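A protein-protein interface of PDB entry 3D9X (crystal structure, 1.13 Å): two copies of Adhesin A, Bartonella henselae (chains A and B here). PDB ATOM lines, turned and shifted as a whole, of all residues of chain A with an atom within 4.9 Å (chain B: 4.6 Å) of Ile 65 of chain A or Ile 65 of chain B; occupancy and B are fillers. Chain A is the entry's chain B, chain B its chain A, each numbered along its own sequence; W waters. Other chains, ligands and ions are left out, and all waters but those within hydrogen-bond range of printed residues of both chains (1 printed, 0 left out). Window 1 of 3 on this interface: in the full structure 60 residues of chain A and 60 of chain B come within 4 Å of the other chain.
Hydrophobic or aromatic side chains of chain B within 4 Å of the printed part of chain A: Leu 60, Leu 62, Ile 65 and Leu 72.
Of the 9 printed residues of chain A, 6 touch a printed residue of chain B.
Among the printed residues, 10 pairs touch across the chains.
Ile 65 of chain A touches Leu 62 of chain B, but with the chains exchanged Leu 62 of chain A does not touch Ile 65 of chain B (6.5 Å).
Lys 66 of chain A touches Leu 62 of chain B, but with the chains exchanged Leu 62 of chain A does not touch Lys 66 of chain B (11.5 Å).
Leu 67 of chain A touches Leu 62 of chain B, but with the chains exchanged Leu 62 of chain A does not touch Leu 67 of chain B (9.4 Å).
Val 70 of chain A touches Leu 72 of chain B, but with the chains exchanged Leu 72 of chain A does not touch Val 70 of chain B (8.9 Å).
8 positions are printed for both chains.
Of the 10 pairs that touch across the chains among the printed residues, 1 has its exchanged pair printed and touching as well.
The backbone NH (N) of Ile 65 of chain B sits at hydrogen-bond distance from the backbone carbonyl oxygen (O) of Leu 72 of chain B, at 2.8 Å.
The backbone carbonyl oxygen (O) of Leu 72 of chain A is in hydrogen-bond range of the backbone NH (N) of Ile 65 of chain A, 2.8 Å away.
Water W1 lies within hydrogen-bond range of OG of Ser 64 of chain A (2.8 Å) and O of Leu 60 of chain B (2.9 Å).
Ile 65 of chain A touches just these residues of chain B: Leu 60 (3.3 Å), Leu 62 (3.8 Å) and Ile 65 (3.6 Å).
Of the printed residues of chain B, Lys 66 of chain A touches Leu 60 (2.9 Å) and Leu 62 (3.0 Å).
Of the printed residues of chain B, Leu 67 of chain A touches Leu 62 (3.0 Å) and Leu 72 (3.5 Å).
Of the printed residues of chain B, Val 70 of chain A touches Leu 72.
Ser 64 of chain B touches none of the printed residues of chain A.
Ile 65 of chain B touches just one residue of chain A: Ile 65.
The nearest printed residue of chain B that does not touch Ile 65 of chain A is Leu 72 of chain B (5.3 Å).
The nearest printed residue of chain A that does not touch Ile 65 of chain B is Leu 67 of chain A (4.7 Å).
O of Ser 64 of chain A lies within hydrogen-bond range of N of Leu 60 of chain B (3.0 Å).
The backbone carbonyl oxygen (O) of Leu 60 of chain B is in hydrogen-bond range of the backbone NH (N) of Lys 66 of chain A (2.9 Å).
O of Lys 66 of chain A lies within hydrogen-bond range of N of Leu 62 of chain B (3.0 Å).
Among the printed residues, pairs that only touch across the chains: Leu 62 of chain A with Leu 60 of chain B (3.7 Å), Ile 65 of chain A with Leu 60 of chain B (3.3 Å), Ile 65 of chain A with Leu 62 of chain B (3.8 Å), Ile 65 of chain A with Ile 65 of chain B (3.6 Å), Leu 67 of chain A with Leu 62 of chain B (3.0 Å), Leu 67 of chain A with Leu 72 of chain B (3.5 Å) and Val 70 of chain A with Leu 72 of chain B (3.98 Å).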
ATOM      1  N   LEU A  62      32.885   5.969  10.991  1.00  0.00           N
ATOM      2  CA  LEU A  62      33.494   5.755   9.685  1.00  0.00           C
ATOM      3  C   LEU A  62      34.391   6.910   9.298  1.00  0.00           C
ATOM      4  O   LEU A  62      34.285   8.010   9.827  1.00  0.00           O
ATOM      5  CB  LEU A  62      32.429   5.588   8.588  1.00  0.00           C
ATOM      6  CG  LEU A  62      31.455   4.429   8.762  1.00  0.00           C
ATOM      7  CD1 LEU A  62      30.340   4.520   7.728  1.00  0.00           C
ATOM      8  CD2 LEU A  62      32.165   3.107   8.664  1.00  0.00           C
ATOM      9  N   LYS A  63      35.241   6.645   8.321  1.00  0.00           N
ATOM     10  CA  LYS A  63      36.027   7.681   7.656  1.00  0.00           C
ATOM     11  C   LYS A  63      35.266   8.313   6.497  1.00  0.00           C
ATOM     12  O   LYS A  63      35.273   9.539   6.336  1.00  0.00           O
ATOM     13  CB  LYS A  63      37.346   7.080   7.162  1.00  0.00           C
ATOM     14  CG  LYS A  63      38.258   8.058   6.446  1.00  0.00           C
ATOM     15  CD  LYS A  63      39.743   7.744   6.634  1.00  0.00           C
ATOM     16  CE  LYS A  63      40.334   8.479   7.835  1.00  0.00           C
ATOM     17  NZ  LYS A  63      41.785   8.199   8.046  1.00  0.00           N
ATOM     18  N   SER A  64      34.604   7.491   5.690  1.00  0.00           N
ATOM     19  CA  SER A  64      33.876   8.013   4.549  1.00  0.00           C
ATOM     20  C   SER A  64      32.854   7.032   4.033  1.00  0.00           C
ATOM     21  O   SER A  64      32.952   5.824   4.259  1.00  0.00           O
ATOM     22  CB  SER A  64      34.832   8.399   3.417  1.00  0.00           C
ATOM     23  OG  SER A  64      35.355   7.264   2.744  1.00  0.00           O
ATOM     24  N   ILE A  65      31.885   7.581   3.314  1.00  0.00           N
ATOM     25  CA  ILE A  65      30.949   6.804   2.519  1.00  0.00           C
ATOM     26  C   ILE A  65      30.829   7.435   1.142  1.00  0.00           C
ATOM     27  O   ILE A  65      30.655   8.651   1.021  1.00  0.00           O
ATOM     28  CB  ILE A  65      29.540   6.761   3.139  1.00  0.00           C
ATOM     29  CG1 ILE A  65      29.622   6.389   4.627  1.00  0.00           C
ATOM     30  CG2 ILE A  65      28.642   5.795   2.378  1.00  0.00           C
ATOM     31  CD1 ILE A  65      28.270   6.324   5.336  1.00  0.00           C
ATOM     32  N   LYS A  66      30.932   6.611   0.105  1.00  0.00           N
ATOM     33  CA  LYS A  66      30.751   7.024  -1.276  1.00  0.00           C
ATOM     34  C   LYS A  66      29.503   6.352  -1.806  1.00  0.00           C
ATOM     35  O   LYS A  66      29.354   5.141  -1.700  1.00  0.00           O
ATOM     36  CB  LYS A  66      31.948   6.610  -2.131  1.00  0.00           C
ATOM     37  CG  LYS A  66      31.858   6.981  -3.605  1.00  0.00           C
ATOM     38  CD  LYS A  66      32.942   6.302  -4.448  1.00  0.00           C
ATOM     39  CE  LYS A  66      32.747   6.591  -5.927  1.00  0.00           C
ATOM     40  NZ  LYS A  66      33.701   5.817  -6.764  1.00  0.00           N
ATOM     41  N   LEU A  67      28.612   7.162  -2.367  1.00  0.00           N
ATOM     42  CA  LEU A  67      27.398   6.692  -3.026  1.00  0.00           C
ATOM     43  C   LEU A  67      27.384   7.365  -4.400  1.00  0.00           C
ATOM     44  O   LEU A  67      26.830   8.429  -4.586  1.00  0.00           O
ATOM     45  CB  LEU A  67      26.132   7.019  -2.221  1.00  0.00           C
ATOM     46  CG  LEU A  67      26.136   6.801  -0.700  1.00  0.00           C
ATOM     47  CD1 LEU A  67      24.709   6.698  -0.174  1.00  0.00           C
ATOM     48  CD2 LEU A  67      26.902   5.584  -0.287  1.00  0.00           C
ATOM     49  N   VAL A  70      27.906  11.149  -4.582  1.00  0.00           N
ATOM     50  CA  VAL A  70      27.701  11.666  -3.231  1.00  0.00           C
ATOM     51  C   VAL A  70      28.788  11.130  -2.299  1.00  0.00           C
ATOM     52  O   VAL A  70      29.077   9.933  -2.287  1.00  0.00           O
ATOM     53  CB  VAL A  70      26.305  11.260  -2.722  1.00  0.00           C
ATOM     54  CG1 VAL A  70      26.065  11.784  -1.302  1.00  0.00           C
ATOM     55  CG2 VAL A  70      25.228  11.774  -3.681  1.00  0.00           C
ATOM     56  N   THR A  71      29.411  12.015  -1.540  1.00  0.00           N
ATOM     57  CA  THR A  71      30.424  11.642  -0.559  1.00  0.00           C
ATOM     58  C   THR A  71      30.073  12.250   0.793  1.00  0.00           C
ATOM     59  O   THR A  71      29.814  13.444   0.900  1.00  0.00           O
ATOM     60  CB  THR A  71      31.826  12.145  -0.961  1.00  0.00           C
ATOM     61  OG1 THR A  71      32.193  11.632  -2.244  1.00  0.00           O
ATOM     62  CG2 THR A  71      32.864  11.727   0.072  1.00  0.00           C
ATOM     63  N   LEU A  72      30.098  11.405   1.825  1.00  0.00           N
ATOM     64  CA  LEU A  72      30.005  11.843   3.204  1.00  0.00           C
ATOM     65  C   LEU A  72      31.311  11.488   3.868  1.00  0.00           C
ATOM     66  O   LEU A  72      31.740  10.336   3.818  1.00  0.00           O
ATOM     67  CB  LEU A  72      28.831  11.141   3.884  1.00  0.00           C
ATOM     68  CG  LEU A  72      28.580  11.513   5.342  1.00  0.00           C
ATOM     69  CD1 LEU A  72      28.091  12.934   5.423  1.00  0.00           C
ATOM     70  CD2 LEU A  72      27.585  10.577   5.984  1.00  0.00           C
ATOM     71  N   LEU B  60      33.236   3.095   3.166  1.00  0.00           N
ATOM     72  CA  LEU B  60      32.223   2.240   2.564  1.00  0.00           C
ATOM     73  C   LEU B  60      31.794   2.787   1.224  1.00  0.00           C
ATOM     74  O   LEU B  60      31.798   3.997   0.995  1.00  0.00           O
ATOM     75  CB  LEU B  60      30.983   2.130   3.450  1.00  0.00           C
ATOM     76  CG  LEU B  60      31.165   1.363   4.763  1.00  0.00           C
ATOM     77  CD1 LEU B  60      29.923   1.489   5.616  1.00  0.00           C
ATOM     78  CD2 LEU B  60      31.495  -0.096   4.516  1.00  0.00           C
ATOM     79  N   LEU B  62      28.285   2.478  -0.907  1.00  0.00           N
ATOM     80  CA  LEU B  62      26.904   2.058  -0.675  1.00  0.00           C
ATOM     81  C   LEU B  62      25.973   2.630  -1.718  1.00  0.00           C
ATOM     82  O   LEU B  62      26.305   3.584  -2.410  1.00  0.00           O
ATOM     83  CB  LEU B  62      26.440   2.515   0.708  1.00  0.00           C
ATOM     84  CG  LEU B  62      27.188   1.973   1.922  1.00  0.00           C
ATOM     85  CD1 LEU B  62      26.693   2.636   3.211  1.00  0.00           C
ATOM     86  CD2 LEU B  62      27.084   0.445   2.004  1.00  0.00           C
ATOM     87  N   SER B  64      22.498   3.083  -0.582  1.00  0.00           N
ATOM     88  CA  SER B  64      21.600   3.913   0.221  1.00  0.00           C
ATOM     89  C   SER B  64      21.742   3.616   1.688  1.00  0.00           C
ATOM     90  O   SER B  64      22.189   2.545   2.096  1.00  0.00           O
ATOM     91  CB  SER B  64      20.125   3.757  -0.211  1.00  0.00           C
ATOM     92  OG  SER B  64      19.569   2.520   0.220  1.00  0.00           O
ATOM     93  N   ILE B  65      21.305   4.588   2.471  1.00  0.00           N
ATOM     94  CA  ILE B  65      21.203   4.477   3.918  1.00  0.00           C
ATOM     95  C   ILE B  65      19.881   5.101   4.346  1.00  0.00           C
ATOM     96  O   ILE B  65      19.558   6.215   3.947  1.00  0.00           O
ATOM     97  CB  ILE B  65      22.339   5.216   4.672  1.00  0.00           C
ATOM     98  CG1 ILE B  65      23.706   4.895   4.073  1.00  0.00           C
ATOM     99  CG2 ILE B  65      22.276   4.864   6.152  1.00  0.00           C
ATOM    100  CD1 ILE B  65      24.797   5.821   4.554  1.00  0.00           C
ATOM    101  N   LYS B  66      19.122   4.370   5.143  1.00  0.00           N
ATOM    102  CA  LYS B  66      17.899   4.852   5.753  1.00  0.00           C
ATOM    103  C   LYS B  66      18.089   4.965   7.249  1.00  0.00           C
ATOM    104  O   LYS B  66      18.490   3.984   7.886  1.00  0.00           O
ATOM    105  CB  LYS B  66      16.761   3.885   5.452  1.00  0.00           C
ATOM    106  CG  LYS B  66      15.437   4.298   6.076  1.00  0.00           C
ATOM    107  CD  LYS B  66      14.359   3.261   5.873  1.00  0.00           C
ATOM    108  CE  LYS B  66      13.138   3.551   6.691  1.00  0.00           C
ATOM    109  NZ  LYS B  66      12.545   4.831   6.266  1.00  0.00           N
ATOM    110  N   LEU B  67      17.781   6.147   7.775  1.00  0.00           N
ATOM    111  CA  LEU B  67      17.841   6.427   9.204  1.00  0.00           C
ATOM    112  C   LEU B  67      16.499   7.060   9.542  1.00  0.00           C
ATOM    113  O   LEU B  67      16.333   8.272   9.522  1.00  0.00           O
ATOM    114  CB  LEU B  67      19.038   7.306   9.568  1.00  0.00           C
ATOM    115  CG  LEU B  67      20.360   6.970   8.895  1.00  0.00           C
ATOM    116  CD1 LEU B  67      20.548   7.770   7.591  1.00  0.00           C
ATOM    117  CD2 LEU B  67      21.537   7.227   9.825  1.00  0.00           C
ATOM    118  N   VAL B  70      15.269   9.969   7.361  1.00  0.00           N
ATOM    119  CA  VAL B  70      16.442  10.493   6.665  1.00  0.00           C
ATOM    120  C   VAL B  70      16.942   9.413   5.730  1.00  0.00           C
ATOM    121  O   VAL B  70      17.150   8.277   6.141  1.00  0.00           O
ATOM    122  CB  VAL B  70      17.530  10.882   7.668  1.00  0.00           C
ATOM    123  CG1 VAL B  70      18.777  11.373   6.956  1.00  0.00           C
ATOM    124  CG2 VAL B  70      17.015  11.919   8.630  1.00  0.00           C
ATOM    125  N   THR B  71      17.170   9.766   4.467  1.00  0.00           N
ATOM    126  CA  THR B  71      17.764   8.858   3.490  1.00  0.00           C
ATOM    127  C   THR B  71      18.956   9.528   2.820  1.00  0.00           C
ATOM    128  O   THR B  71      18.868  10.692   2.415  1.00  0.00           O
ATOM    129  CB  THR B  71      16.745   8.453   2.396  1.00  0.00           C
ATOM    130  OG1 THR B  71      15.634   7.809   3.010  1.00  0.00           O
ATOM    131  CG2 THR B  71      17.341   7.515   1.391  1.00  0.00           C
ATOM    132  N   LEU B  72      20.059   8.793   2.704  1.00  0.00           N
ATOM    133  CA  LEU B  72      21.204   9.211   1.899  1.00  0.00           C
ATOM    134  C   LEU B  72      21.357   8.182   0.795  1.00  0.00           C
ATOM    135  O   LEU B  72      21.415   6.988   1.065  1.00  0.00           O
ATOM    136  CB  LEU B  72      22.465   9.298   2.750  1.00  0.00           C
ATOM    137  CG  LEU B  72      23.696   9.879   2.052  1.00  0.00           C
ATOM    138  CD1 LEU B  72      23.497  11.345   1.709  1.00  0.00           C
ATOM    139  CD2 LEU B  72      24.928   9.711   2.896  1.00  0.00           C
HETATM  140  O   HOH W   1      34.201   5.538   0.862  1.00  0.00           O
